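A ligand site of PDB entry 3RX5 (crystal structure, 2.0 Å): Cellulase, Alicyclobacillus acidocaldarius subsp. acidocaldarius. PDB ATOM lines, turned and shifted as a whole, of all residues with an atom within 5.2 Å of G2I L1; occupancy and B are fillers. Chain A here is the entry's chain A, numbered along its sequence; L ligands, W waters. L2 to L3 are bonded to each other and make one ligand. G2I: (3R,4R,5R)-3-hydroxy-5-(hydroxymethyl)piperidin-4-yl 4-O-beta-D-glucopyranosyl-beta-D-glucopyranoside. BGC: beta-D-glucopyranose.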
ATOM      1  N   ASP A 143       5.576  -0.467 -20.664  1.00  0.00           N
ATOM      2  CA  ASP A 143       5.313  -1.624 -19.834  1.00  0.00           C
ATOM      3  C   ASP A 143       5.773  -1.478 -18.398  1.00  0.00           C
ATOM      4  O   ASP A 143       5.046  -1.836 -17.504  1.00  0.00           O
ATOM      5  CB  ASP A 143       6.048  -2.823 -20.455  1.00  0.00           C
ATOM      6  CG  ASP A 143       5.738  -4.178 -19.852  1.00  0.00           C
ATOM      7  OD1 ASP A 143       4.570  -4.596 -19.938  1.00  0.00           O
ATOM      8  OD2 ASP A 143       6.710  -4.904 -19.488  1.00  0.00           O
ATOM      9  N   ALA A 144       6.995  -0.992 -18.190  1.00  0.00           N
ATOM     10  CA  ALA A 144       7.612  -1.095 -16.877  1.00  0.00           C
ATOM     11  C   ALA A 144       8.752  -0.094 -16.675  1.00  0.00           C
ATOM     12  O   ALA A 144       8.531   1.118 -16.764  1.00  0.00           O
ATOM     13  CB  ALA A 144       8.152  -2.544 -16.752  1.00  0.00           C
ATOM     14  N   GLY A 145       9.953  -0.602 -16.388  1.00  0.00           N
ATOM     15  CA  GLY A 145      11.159   0.207 -16.259  1.00  0.00           C
ATOM     16  C   GLY A 145      11.765   0.466 -17.636  1.00  0.00           C
ATOM     17  O   GLY A 145      12.622   1.315 -17.779  1.00  0.00           O
ATOM     18  N   ASP A 146      11.295  -0.246 -18.660  1.00  0.00           N
ATOM     19  CA  ASP A 146      11.706  -0.070 -20.065  1.00  0.00           C
ATOM     20  C   ASP A 146      10.556   0.607 -20.847  1.00  0.00           C
ATOM     21  O   ASP A 146       9.489   0.836 -20.308  1.00  0.00           O
ATOM     22  CB  ASP A 146      12.079  -1.416 -20.680  1.00  0.00           C
ATOM     23  CG  ASP A 146      10.896  -2.317 -20.942  1.00  0.00           C
ATOM     24  OD1 ASP A 146      10.159  -2.618 -19.966  1.00  0.00           O
ATOM     25  OD2 ASP A 146      10.716  -2.740 -22.093  1.00  0.00           O
ATOM     26  N   TYR A 150       3.947  -4.219 -24.739  1.00  0.00           N
ATOM     27  CA  TYR A 150       3.739  -5.643 -24.949  1.00  0.00           C
ATOM     28  C   TYR A 150       2.281  -5.979 -24.726  1.00  0.00           C
ATOM     29  O   TYR A 150       1.732  -5.678 -23.670  1.00  0.00           O
ATOM     30  CB  TYR A 150       4.629  -6.460 -23.987  1.00  0.00           C
ATOM     31  CG  TYR A 150       6.073  -6.013 -23.881  1.00  0.00           C
ATOM     32  CD1 TYR A 150       6.435  -4.949 -23.074  1.00  0.00           C
ATOM     33  CD2 TYR A 150       7.084  -6.740 -24.495  1.00  0.00           C
ATOM     34  CE1 TYR A 150       7.775  -4.587 -22.911  1.00  0.00           C
ATOM     35  CE2 TYR A 150       8.423  -6.372 -24.369  1.00  0.00           C
ATOM     36  CZ  TYR A 150       8.769  -5.308 -23.550  1.00  0.00           C
ATOM     37  OH  TYR A 150      10.091  -4.982 -23.417  1.00  0.00           O
ATOM     38  N   PHE A 221      17.138  -3.006 -25.362  1.00  0.00           N
ATOM     39  CA  PHE A 221      16.920  -2.120 -24.243  1.00  0.00           C
ATOM     40  C   PHE A 221      17.927  -0.975 -24.291  1.00  0.00           C
ATOM     41  O   PHE A 221      19.120  -1.223 -24.439  1.00  0.00           O
ATOM     42  CB  PHE A 221      17.075  -2.842 -22.901  1.00  0.00           C
ATOM     43  CG  PHE A 221      16.014  -3.869 -22.620  1.00  0.00           C
ATOM     44  CD1 PHE A 221      14.682  -3.505 -22.496  1.00  0.00           C
ATOM     45  CD2 PHE A 221      16.362  -5.200 -22.437  1.00  0.00           C
ATOM     46  CE1 PHE A 221      13.703  -4.462 -22.196  1.00  0.00           C
ATOM     47  CE2 PHE A 221      15.391  -6.153 -22.106  1.00  0.00           C
ATOM     48  CZ  PHE A 221      14.074  -5.778 -21.995  1.00  0.00           C
ATOM     49  N   GLY A 298      11.846  -7.613 -23.821  1.00  0.00           N
ATOM     50  CA  GLY A 298      11.021  -8.560 -23.068  1.00  0.00           C
ATOM     51  C   GLY A 298      10.304  -9.557 -23.957  1.00  0.00           C
ATOM     52  O   GLY A 298       9.568  -9.163 -24.854  1.00  0.00           O
ATOM     53  N   GLU A 299      10.555 -10.845 -23.754  1.00  0.00           N
ATOM     54  CA  GLU A 299       9.938 -11.847 -24.598  1.00  0.00           C
ATOM     55  C   GLU A 299       8.473 -12.116 -24.309  1.00  0.00           C
ATOM     56  O   GLU A 299       7.705 -12.327 -25.268  1.00  0.00           O
ATOM     57  CB  GLU A 299      10.728 -13.140 -24.578  1.00  0.00           C
ATOM     58  CG  GLU A 299      10.316 -14.114 -25.656  1.00  0.00           C
ATOM     59  CD  GLU A 299      11.230 -15.313 -25.733  1.00  0.00           C
ATOM     60  OE1 GLU A 299      11.200 -16.132 -24.784  1.00  0.00           O
ATOM     61  OE2 GLU A 299      12.024 -15.389 -26.696  1.00  0.00           O
ATOM     62  N   TYR A 300       8.096 -12.199 -23.013  1.00  0.00           N
ATOM     63  CA  TYR A 300       6.735 -12.574 -22.570  1.00  0.00           C
ATOM     64  C   TYR A 300       6.308 -13.829 -23.304  1.00  0.00           C
ATOM     65  O   TYR A 300       5.258 -13.874 -23.937  1.00  0.00           O
ATOM     66  CB  TYR A 300       5.727 -11.429 -22.749  1.00  0.00           C
ATOM     67  CG  TYR A 300       5.910 -10.331 -21.722  1.00  0.00           C
ATOM     68  CD1 TYR A 300       5.532 -10.522 -20.396  1.00  0.00           C
ATOM     69  CD2 TYR A 300       6.455  -9.111 -22.083  1.00  0.00           C
ATOM     70  CE1 TYR A 300       5.699  -9.514 -19.451  1.00  0.00           C
ATOM     71  CE2 TYR A 300       6.615  -8.095 -21.149  1.00  0.00           C
ATOM     72  CZ  TYR A 300       6.199  -8.291 -19.845  1.00  0.00           C
ATOM     73  OH  TYR A 300       6.409  -7.292 -18.927  1.00  0.00           O
ATOM     74  N   TRP A 343       0.743 -12.924 -15.408  1.00  0.00           N
ATOM     75  CA  TRP A 343       0.546 -12.536 -16.814  1.00  0.00           C
ATOM     76  C   TRP A 343       0.503 -13.717 -17.798  1.00  0.00           C
ATOM     77  O   TRP A 343      -0.115 -13.610 -18.859  1.00  0.00           O
ATOM     78  CB  TRP A 343       1.644 -11.541 -17.258  1.00  0.00           C
ATOM     79  CG  TRP A 343       3.041 -12.080 -17.167  1.00  0.00           C
ATOM     80  CD1 TRP A 343       3.912 -11.901 -16.125  1.00  0.00           C
ATOM     81  CD2 TRP A 343       3.743 -12.883 -18.145  1.00  0.00           C
ATOM     82  NE1 TRP A 343       5.118 -12.525 -16.401  1.00  0.00           N
ATOM     83  CE2 TRP A 343       5.050 -13.089 -17.662  1.00  0.00           C
ATOM     84  CE3 TRP A 343       3.418 -13.356 -19.446  1.00  0.00           C
ATOM     85  CZ2 TRP A 343       6.003 -13.851 -18.365  1.00  0.00           C
ATOM     86  CZ3 TRP A 343       4.362 -14.136 -20.128  1.00  0.00           C
ATOM     87  CH2 TRP A 343       5.624 -14.400 -19.571  1.00  0.00           C
ATOM     88  N   ILE A 400       9.271 -15.139  -6.067  1.00  0.00           N
ATOM     89  CA  ILE A 400       9.891 -15.147  -7.399  1.00  0.00           C
ATOM     90  C   ILE A 400       9.843 -13.755  -7.980  1.00  0.00           C
ATOM     91  O   ILE A 400       9.445 -12.799  -7.297  1.00  0.00           O
ATOM     92  CB  ILE A 400       9.157 -16.198  -8.315  1.00  0.00           C
ATOM     93  CG1 ILE A 400       7.628 -15.870  -8.455  1.00  0.00           C
ATOM     94  CG2 ILE A 400       9.399 -17.625  -7.770  1.00  0.00           C
ATOM     95  CD1 ILE A 400       6.867 -16.590  -9.577  1.00  0.00           C
ATOM     96  N   TRP A 401      10.224 -13.619  -9.250  1.00  0.00           N
ATOM     97  CA  TRP A 401      10.193 -12.338  -9.957  1.00  0.00           C
ATOM     98  C   TRP A 401       8.728 -11.878  -9.956  1.00  0.00           C
ATOM     99  O   TRP A 401       7.852 -12.668 -10.328  1.00  0.00           O
ATOM    100  CB  TRP A 401      10.657 -12.535 -11.409  1.00  0.00           C
ATOM    101  CG  TRP A 401      11.068 -11.269 -12.100  1.00  0.00           C
ATOM    102  CD1 TRP A 401      10.377 -10.103 -12.177  1.00  0.00           C
ATOM    103  CD2 TRP A 401      12.228 -11.114 -12.931  1.00  0.00           C
ATOM    104  NE1 TRP A 401      11.058  -9.193 -12.950  1.00  0.00           N
ATOM    105  CE2 TRP A 401      12.185  -9.806 -13.453  1.00  0.00           C
ATOM    106  CE3 TRP A 401      13.252 -11.981 -13.350  1.00  0.00           C
ATOM    107  CZ2 TRP A 401      13.151  -9.322 -14.343  1.00  0.00           C
ATOM    108  CZ3 TRP A 401      14.237 -11.491 -14.193  1.00  0.00           C
ATOM    109  CH2 TRP A 401      14.164 -10.186 -14.707  1.00  0.00           C
ATOM    110  N   GLN A 487      17.981 -13.216  -9.835  1.00  0.00           N
ATOM    111  CA  GLN A 487      17.984 -13.085 -11.280  1.00  0.00           C
ATOM    112  C   GLN A 487      18.575 -11.814 -11.897  1.00  0.00           C
ATOM    113  O   GLN A 487      18.239 -11.463 -13.025  1.00  0.00           O
ATOM    114  CB  GLN A 487      16.641 -13.520 -11.888  1.00  0.00           C
ATOM    115  CG  GLN A 487      16.314 -15.001 -11.626  1.00  0.00           C
ATOM    116  CD  GLN A 487      14.895 -15.374 -11.929  1.00  0.00           C
ATOM    117  OE1 GLN A 487      13.946 -14.772 -11.408  1.00  0.00           O
ATOM    118  NE2 GLN A 487      14.702 -16.465 -12.662  1.00  0.00           N
ATOM    119  N   TYR A 511      16.859  -5.254 -11.424  1.00  0.00           N
ATOM    120  CA  TYR A 511      15.602  -5.372 -12.175  1.00  0.00           C
ATOM    121  C   TYR A 511      14.774  -6.588 -11.787  1.00  0.00           C
ATOM    122  O   TYR A 511      13.565  -6.590 -12.022  1.00  0.00           O
ATOM    123  CB  TYR A 511      15.872  -5.352 -13.692  1.00  0.00           C
ATOM    124  CG  TYR A 511      16.944  -6.310 -14.152  1.00  0.00           C
ATOM    125  CD1 TYR A 511      16.664  -7.653 -14.377  1.00  0.00           C
ATOM    126  CD2 TYR A 511      18.242  -5.872 -14.395  1.00  0.00           C
ATOM    127  CE1 TYR A 511      17.648  -8.539 -14.839  1.00  0.00           C
ATOM    128  CE2 TYR A 511      19.221  -6.731 -14.882  1.00  0.00           C
ATOM    129  CZ  TYR A 511      18.923  -8.064 -15.097  1.00  0.00           C
ATOM    130  OH  TYR A 511      19.889  -8.930 -15.551  1.00  0.00           O
ATOM    131  N   GLU A 515      12.088  -3.712 -10.200  1.00  0.00           N
ATOM    132  CA  GLU A 515      11.469  -3.059 -11.361  1.00  0.00           C
ATOM    133  C   GLU A 515      10.025  -2.761 -10.973  1.00  0.00           C
ATOM    134  O   GLU A 515       9.548  -3.212  -9.938  1.00  0.00           O
ATOM    135  CB  GLU A 515      11.515  -3.956 -12.631  1.00  0.00           C
ATOM    136  CG  GLU A 515      11.314  -3.142 -13.910  1.00  0.00           C
ATOM    137  CD  GLU A 515      11.822  -3.695 -15.224  1.00  0.00           C
ATOM    138  OE1 GLU A 515      12.236  -4.880 -15.277  1.00  0.00           O
ATOM    139  OE2 GLU A 515      11.789  -2.947 -16.216  1.00  0.00           O
ATOM    140  N   VAL A 516       9.335  -2.003 -11.816  1.00  0.00           N
ATOM    141  CA  VAL A 516       7.930  -1.615 -11.673  1.00  0.00           C
ATOM    142  C   VAL A 516       7.243  -2.151 -12.945  1.00  0.00           C
ATOM    143  O   VAL A 516       7.956  -2.505 -13.883  1.00  0.00           O
ATOM    144  CB  VAL A 516       7.797  -0.060 -11.538  1.00  0.00           C
ATOM    145  CG1 VAL A 516       8.473   0.445 -10.266  1.00  0.00           C
ATOM    146  CG2 VAL A 516       8.354   0.672 -12.780  1.00  0.00           C
ATOM    147  N   ALA A 517       5.908  -2.236 -12.976  1.00  0.00           N
ATOM    148  CA  ALA A 517       5.201  -2.736 -14.168  1.00  0.00           C
ATOM    149  C   ALA A 517       3.744  -2.387 -14.070  1.00  0.00           C
ATOM    150  O   ALA A 517       3.174  -2.407 -12.972  1.00  0.00           O
ATOM    151  CB  ALA A 517       5.367  -4.258 -14.306  1.00  0.00           C
ATOM    152  N   TYR A 519       1.221  -4.081 -14.883  1.00  0.00           N
ATOM    153  CA  TYR A 519       0.476  -5.261 -14.421  1.00  0.00           C
ATOM    154  C   TYR A 519       0.863  -5.686 -12.965  1.00  0.00           C
ATOM    155  O   TYR A 519       0.441  -6.755 -12.516  1.00  0.00           O
ATOM    156  CB  TYR A 519       0.586  -6.419 -15.426  1.00  0.00           C
ATOM    157  CG  TYR A 519       2.038  -6.824 -15.680  1.00  0.00           C
ATOM    158  CD1 TYR A 519       2.597  -7.917 -15.036  1.00  0.00           C
ATOM    159  CD2 TYR A 519       2.813  -6.132 -16.612  1.00  0.00           C
ATOM    160  CE1 TYR A 519       3.908  -8.316 -15.284  1.00  0.00           C
ATOM    161  CE2 TYR A 519       4.140  -6.520 -16.873  1.00  0.00           C
ATOM    162  CZ  TYR A 519       4.674  -7.613 -16.212  1.00  0.00           C
ATOM    163  OH  TYR A 519       5.982  -7.979 -16.428  1.00  0.00           O
ATOM    164  N   TRP A 520       1.686  -4.880 -12.272  1.00  0.00           N
ATOM    165  CA  TRP A 520       2.010  -5.013 -10.859  1.00  0.00           C
ATOM    166  C   TRP A 520       1.213  -3.919 -10.119  1.00  0.00           C
ATOM    167  O   TRP A 520       0.694  -4.167  -9.029  1.00  0.00           O
ATOM    168  CB  TRP A 520       3.520  -4.936 -10.580  1.00  0.00           C
ATOM    169  CG  TRP A 520       4.307  -6.092 -11.122  1.00  0.00           C
ATOM    170  CD1 TRP A 520       3.807  -7.270 -11.616  1.00  0.00           C
ATOM    171  CD2 TRP A 520       5.730  -6.159 -11.293  1.00  0.00           C
ATOM    172  NE1 TRP A 520       4.834  -8.078 -12.046  1.00  0.00           N
ATOM    173  CE2 TRP A 520       6.027  -7.417 -11.872  1.00  0.00           C
ATOM    174  CE3 TRP A 520       6.783  -5.270 -11.028  1.00  0.00           C
ATOM    175  CZ2 TRP A 520       7.341  -7.811 -12.172  1.00  0.00           C
ATOM    176  CZ3 TRP A 520       8.075  -5.640 -11.377  1.00  0.00           C
ATOM    177  CH2 TRP A 520       8.336  -6.899 -11.921  1.00  0.00           C
HETATM  178  O61 G2I L   1      10.519  -7.091 -14.965  1.00  0.00           O
HETATM  179  C61 G2I L   1       9.244  -6.564 -15.400  1.00  0.00           C
HETATM  180  C51 G2I L   1       9.208  -6.547 -16.946  1.00  0.00           C
HETATM  181  C71 G2I L   1      10.027  -5.297 -17.491  1.00  0.00           C
HETATM  182  N11 G2I L   1       9.695  -5.089 -18.948  1.00  0.00           N
HETATM  183  C21 G2I L   1      10.481  -6.210 -19.652  1.00  0.00           C
HETATM  184  C31 G2I L   1       9.693  -7.541 -19.246  1.00  0.00           C
HETATM  185  O31 G2I L   1      10.266  -8.681 -19.820  1.00  0.00           O
HETATM  186  C41 G2I L   1       9.746  -7.838 -17.690  1.00  0.00           C
HETATM  187  O41 G2I L   1       8.790  -8.930 -17.454  1.00  0.00           O
HETATM  188  C12 G2I L   1       9.273  -9.862 -16.533  1.00  0.00           C
HETATM  189  C22 G2I L   1       8.099 -10.767 -16.018  1.00  0.00           C
HETATM  190  O22 G2I L   1       7.422  -9.896 -15.199  1.00  0.00           O
HETATM  191  C32 G2I L   1       8.765 -11.924 -15.215  1.00  0.00           C
HETATM  192  O32 G2I L   1       7.705 -12.856 -14.781  1.00  0.00           O
HETATM  193  O52 G2I L   1      10.194 -10.664 -17.305  1.00  0.00           O
HETATM  194  C52 G2I L   1      10.892 -11.641 -16.553  1.00  0.00           C
HETATM  195  C62 G2I L   1      12.300 -11.989 -17.307  1.00  0.00           C
HETATM  196  O62 G2I L   1      11.877 -12.771 -18.374  1.00  0.00           O
HETATM  197  C42 G2I L   1       9.872 -12.692 -16.138  1.00  0.00           C
HETATM  198  O42 G2I L   1      10.633 -13.302 -15.197  1.00  0.00           O
HETATM  199  C13 G2I L   1      10.330 -14.654 -14.984  1.00  0.00           C
HETATM  200  C23 G2I L   1      11.551 -15.589 -14.436  1.00  0.00           C
HETATM  201  O23 G2I L   1      12.505 -15.605 -15.261  1.00  0.00           O
HETATM  202  C33 G2I L   1      11.223 -17.009 -14.063  1.00  0.00           C
HETATM  203  O33 G2I L   1      12.259 -17.660 -13.307  1.00  0.00           O
HETATM  204  C43 G2I L   1       9.987 -16.963 -13.155  1.00  0.00           C
HETATM  205  O43 G2I L   1       9.540 -18.263 -13.194  1.00  0.00           O
HETATM  206  O53 G2I L   1       9.302 -14.772 -14.005  1.00  0.00           O
HETATM  207  C53 G2I L   1       8.788 -16.109 -13.838  1.00  0.00           C
HETATM  208  C63 G2I L   1       7.420 -16.078 -13.058  1.00  0.00           C
HETATM  209  O63 G2I L   1       6.660 -14.963 -13.479  1.00  0.00           O
HETATM  210  C2  BGC L   2      21.158  -5.950 -19.612  1.00  0.00           C
HETATM  211  C3  BGC L   2      19.658  -5.682 -19.785  1.00  0.00           C
HETATM  212  C4  BGC L   2      19.159  -4.681 -18.743  1.00  0.00           C
HETATM  213  C5  BGC L   2      20.053  -3.446 -18.792  1.00  0.00           C
HETATM  214  C6  BGC L   2      19.650  -2.340 -17.817  1.00  0.00           C
HETATM  215  C1  BGC L   2      21.903  -4.615 -19.629  1.00  0.00           C
HETATM  216  O1  BGC L   2      23.330  -4.730 -19.469  1.00  0.00           O
HETATM  217  O2  BGC L   2      21.600  -6.798 -20.678  1.00  0.00           O
HETATM  218  O3  BGC L   2      18.904  -6.906 -19.757  1.00  0.00           O
HETATM  219  O4  BGC L   2      17.849  -4.260 -19.090  1.00  0.00           O
HETATM  220  O5  BGC L   2      21.401  -3.833 -18.548  1.00  0.00           O
HETATM  221  O6  BGC L   2      19.846  -2.837 -16.491  1.00  0.00           O
HETATM  222  C2  BGC L   3      15.577  -3.938 -18.539  1.00  0.00           C
HETATM  223  C3  BGC L   3      14.391  -4.473 -17.750  1.00  0.00           C
HETATM  224  C4  BGC L   3      14.209  -5.930 -18.105  1.00  0.00           C
HETATM  225  C5  BGC L   3      15.467  -6.780 -17.968  1.00  0.00           C
HETATM  226  C6  BGC L   3      15.190  -8.030 -18.801  1.00  0.00           C
HETATM  227  C1  BGC L   3      16.827  -4.762 -18.232  1.00  0.00           C
HETATM  228  O2  BGC L   3      15.802  -2.569 -18.198  1.00  0.00           O
HETATM  229  O3  BGC L   3      13.196  -3.805 -18.164  1.00  0.00           O
HETATM  230  O4  BGC L   3      13.194  -6.483 -17.256  1.00  0.00           O
HETATM  231  O5  BGC L   3      16.595  -6.141 -18.567  1.00  0.00           O
HETATM  232  O6  BGC L   3      15.889  -9.127 -18.235  1.00  0.00           O
HETATM  233  O   HOH W   1      12.808  -9.803 -19.838  1.00  0.00           O
HETATM  234  O   HOH W   2      11.907 -15.957 -10.402  1.00  0.00           O
HETATM  235  O   HOH W   3       8.763 -10.984 -20.260  1.00  0.00           O
HETATM  236  O   HOH W   4       5.531 -10.673 -13.164  1.00  0.00           O
HETATM  237  O   HOH W   5       5.579 -16.163 -15.458  1.00  0.00           O
HETATM  238  O   HOH W   6       3.723 -14.928 -11.990  1.00  0.00           O
HETATM  239  O   HOH W   7       5.671 -13.171 -11.703  1.00  0.00           O
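Water W7 lies within hydrogen-bond range of the backbone carbonyl oxygen of Trp 401 and an oxygen (O63) of G2I L1. Water W3 lies within hydrogen-bond range of O31 of G2I L1 (2.8 Å) and N of Tyr 300 (3.1 Å). Water W4 lies within hydrogen-bond range of an oxygen (O22) of G2I L1 (2.9 Å) and the indole nitrogen of Trp 520 (2.9 Å). Water W2 lies within hydrogen-bond range of the side-chain amide oxygen (OE1) of Gln 487 (2.6 Å), the backbone NH (N) of Trp 401 (3.1 Å) and an oxygen (O33) of G2I L1 (3.4 Å).
The backbone NH (N) of Gly 298 lies within hydrogen-bond range of the side-chain hydroxyl (OH) of Tyr 150 (3.2 Å). The backbone NH (N) of Gly 145 lies within hydrogen-bond range of the side-chain carboxylate (OE2) of Glu 515 (3.0 Å). OH of Tyr 519 is in hydrogen-bond range of OH of Tyr 300 (2.6 Å). OH of Tyr 300 is in hydrogen-bond range of OD2 of Asp 143, 2.5 Å away. The side-chain carboxylate of Asp 146 is in hydrogen-bond range of the side-chain hydroxyl of Tyr 150 (2.7 Å).
An oxygen (O3) of BGC L3 lies within hydrogen-bond range of the side-chain carboxylate of Glu 515. An oxygen (O33) of G2I L1 is in hydrogen-bond range of the side-chain amide nitrogen (NE2) of Gln 487, 2.8 Å away. O41 of G2I L1 lies within hydrogen-bond range of OH of Tyr 300 (3.2 Å). The side-chain hydroxyl (OH) of Tyr 519 is in hydrogen-bond range of an oxygen (O22) of G2I L1 (2.7 Å). A nitrogen (N11) of G2I L1 is in salt-bridge range of the side-chain carboxylate of Asp 143 (3.0 Å). An oxygen (O61) of G2I L1 sits at hydrogen-bond distance from the indole nitrogen (NE1) of Trp 401, at 3.0 Å. An oxygen (O61) of G2I L1 lies within hydrogen-bond range of the side-chain carboxylate of Glu 515 (2.8 Å). The indole nitrogen (NE1) of Trp 343 is in hydrogen-bond range of an oxygen (O32) of G2I L1 (3.1 Å). N11 of G2I L1 lies within salt-bridge range of OD1 of Asp 146, 2.7 Å away.
Merely in contact with G2I L1: Gly 298, Ala 144, Ile 400, Trp 520 and Tyr 150. Hydrophobic or aromatic side chains that line G2I L1: Ala 144, Tyr 300, Trp 343, Ile 400, Trp 401, Tyr 519 and Trp 520. 13 residues have an atom within 4 Å of G2I L1: Asp 143, Ala 144, Asp 146, Tyr 150, Gly 298, Tyr 300, Trp 343, Ile 400, Trp 401, Gln 487, Glu 515, Tyr 519 and Trp 520.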
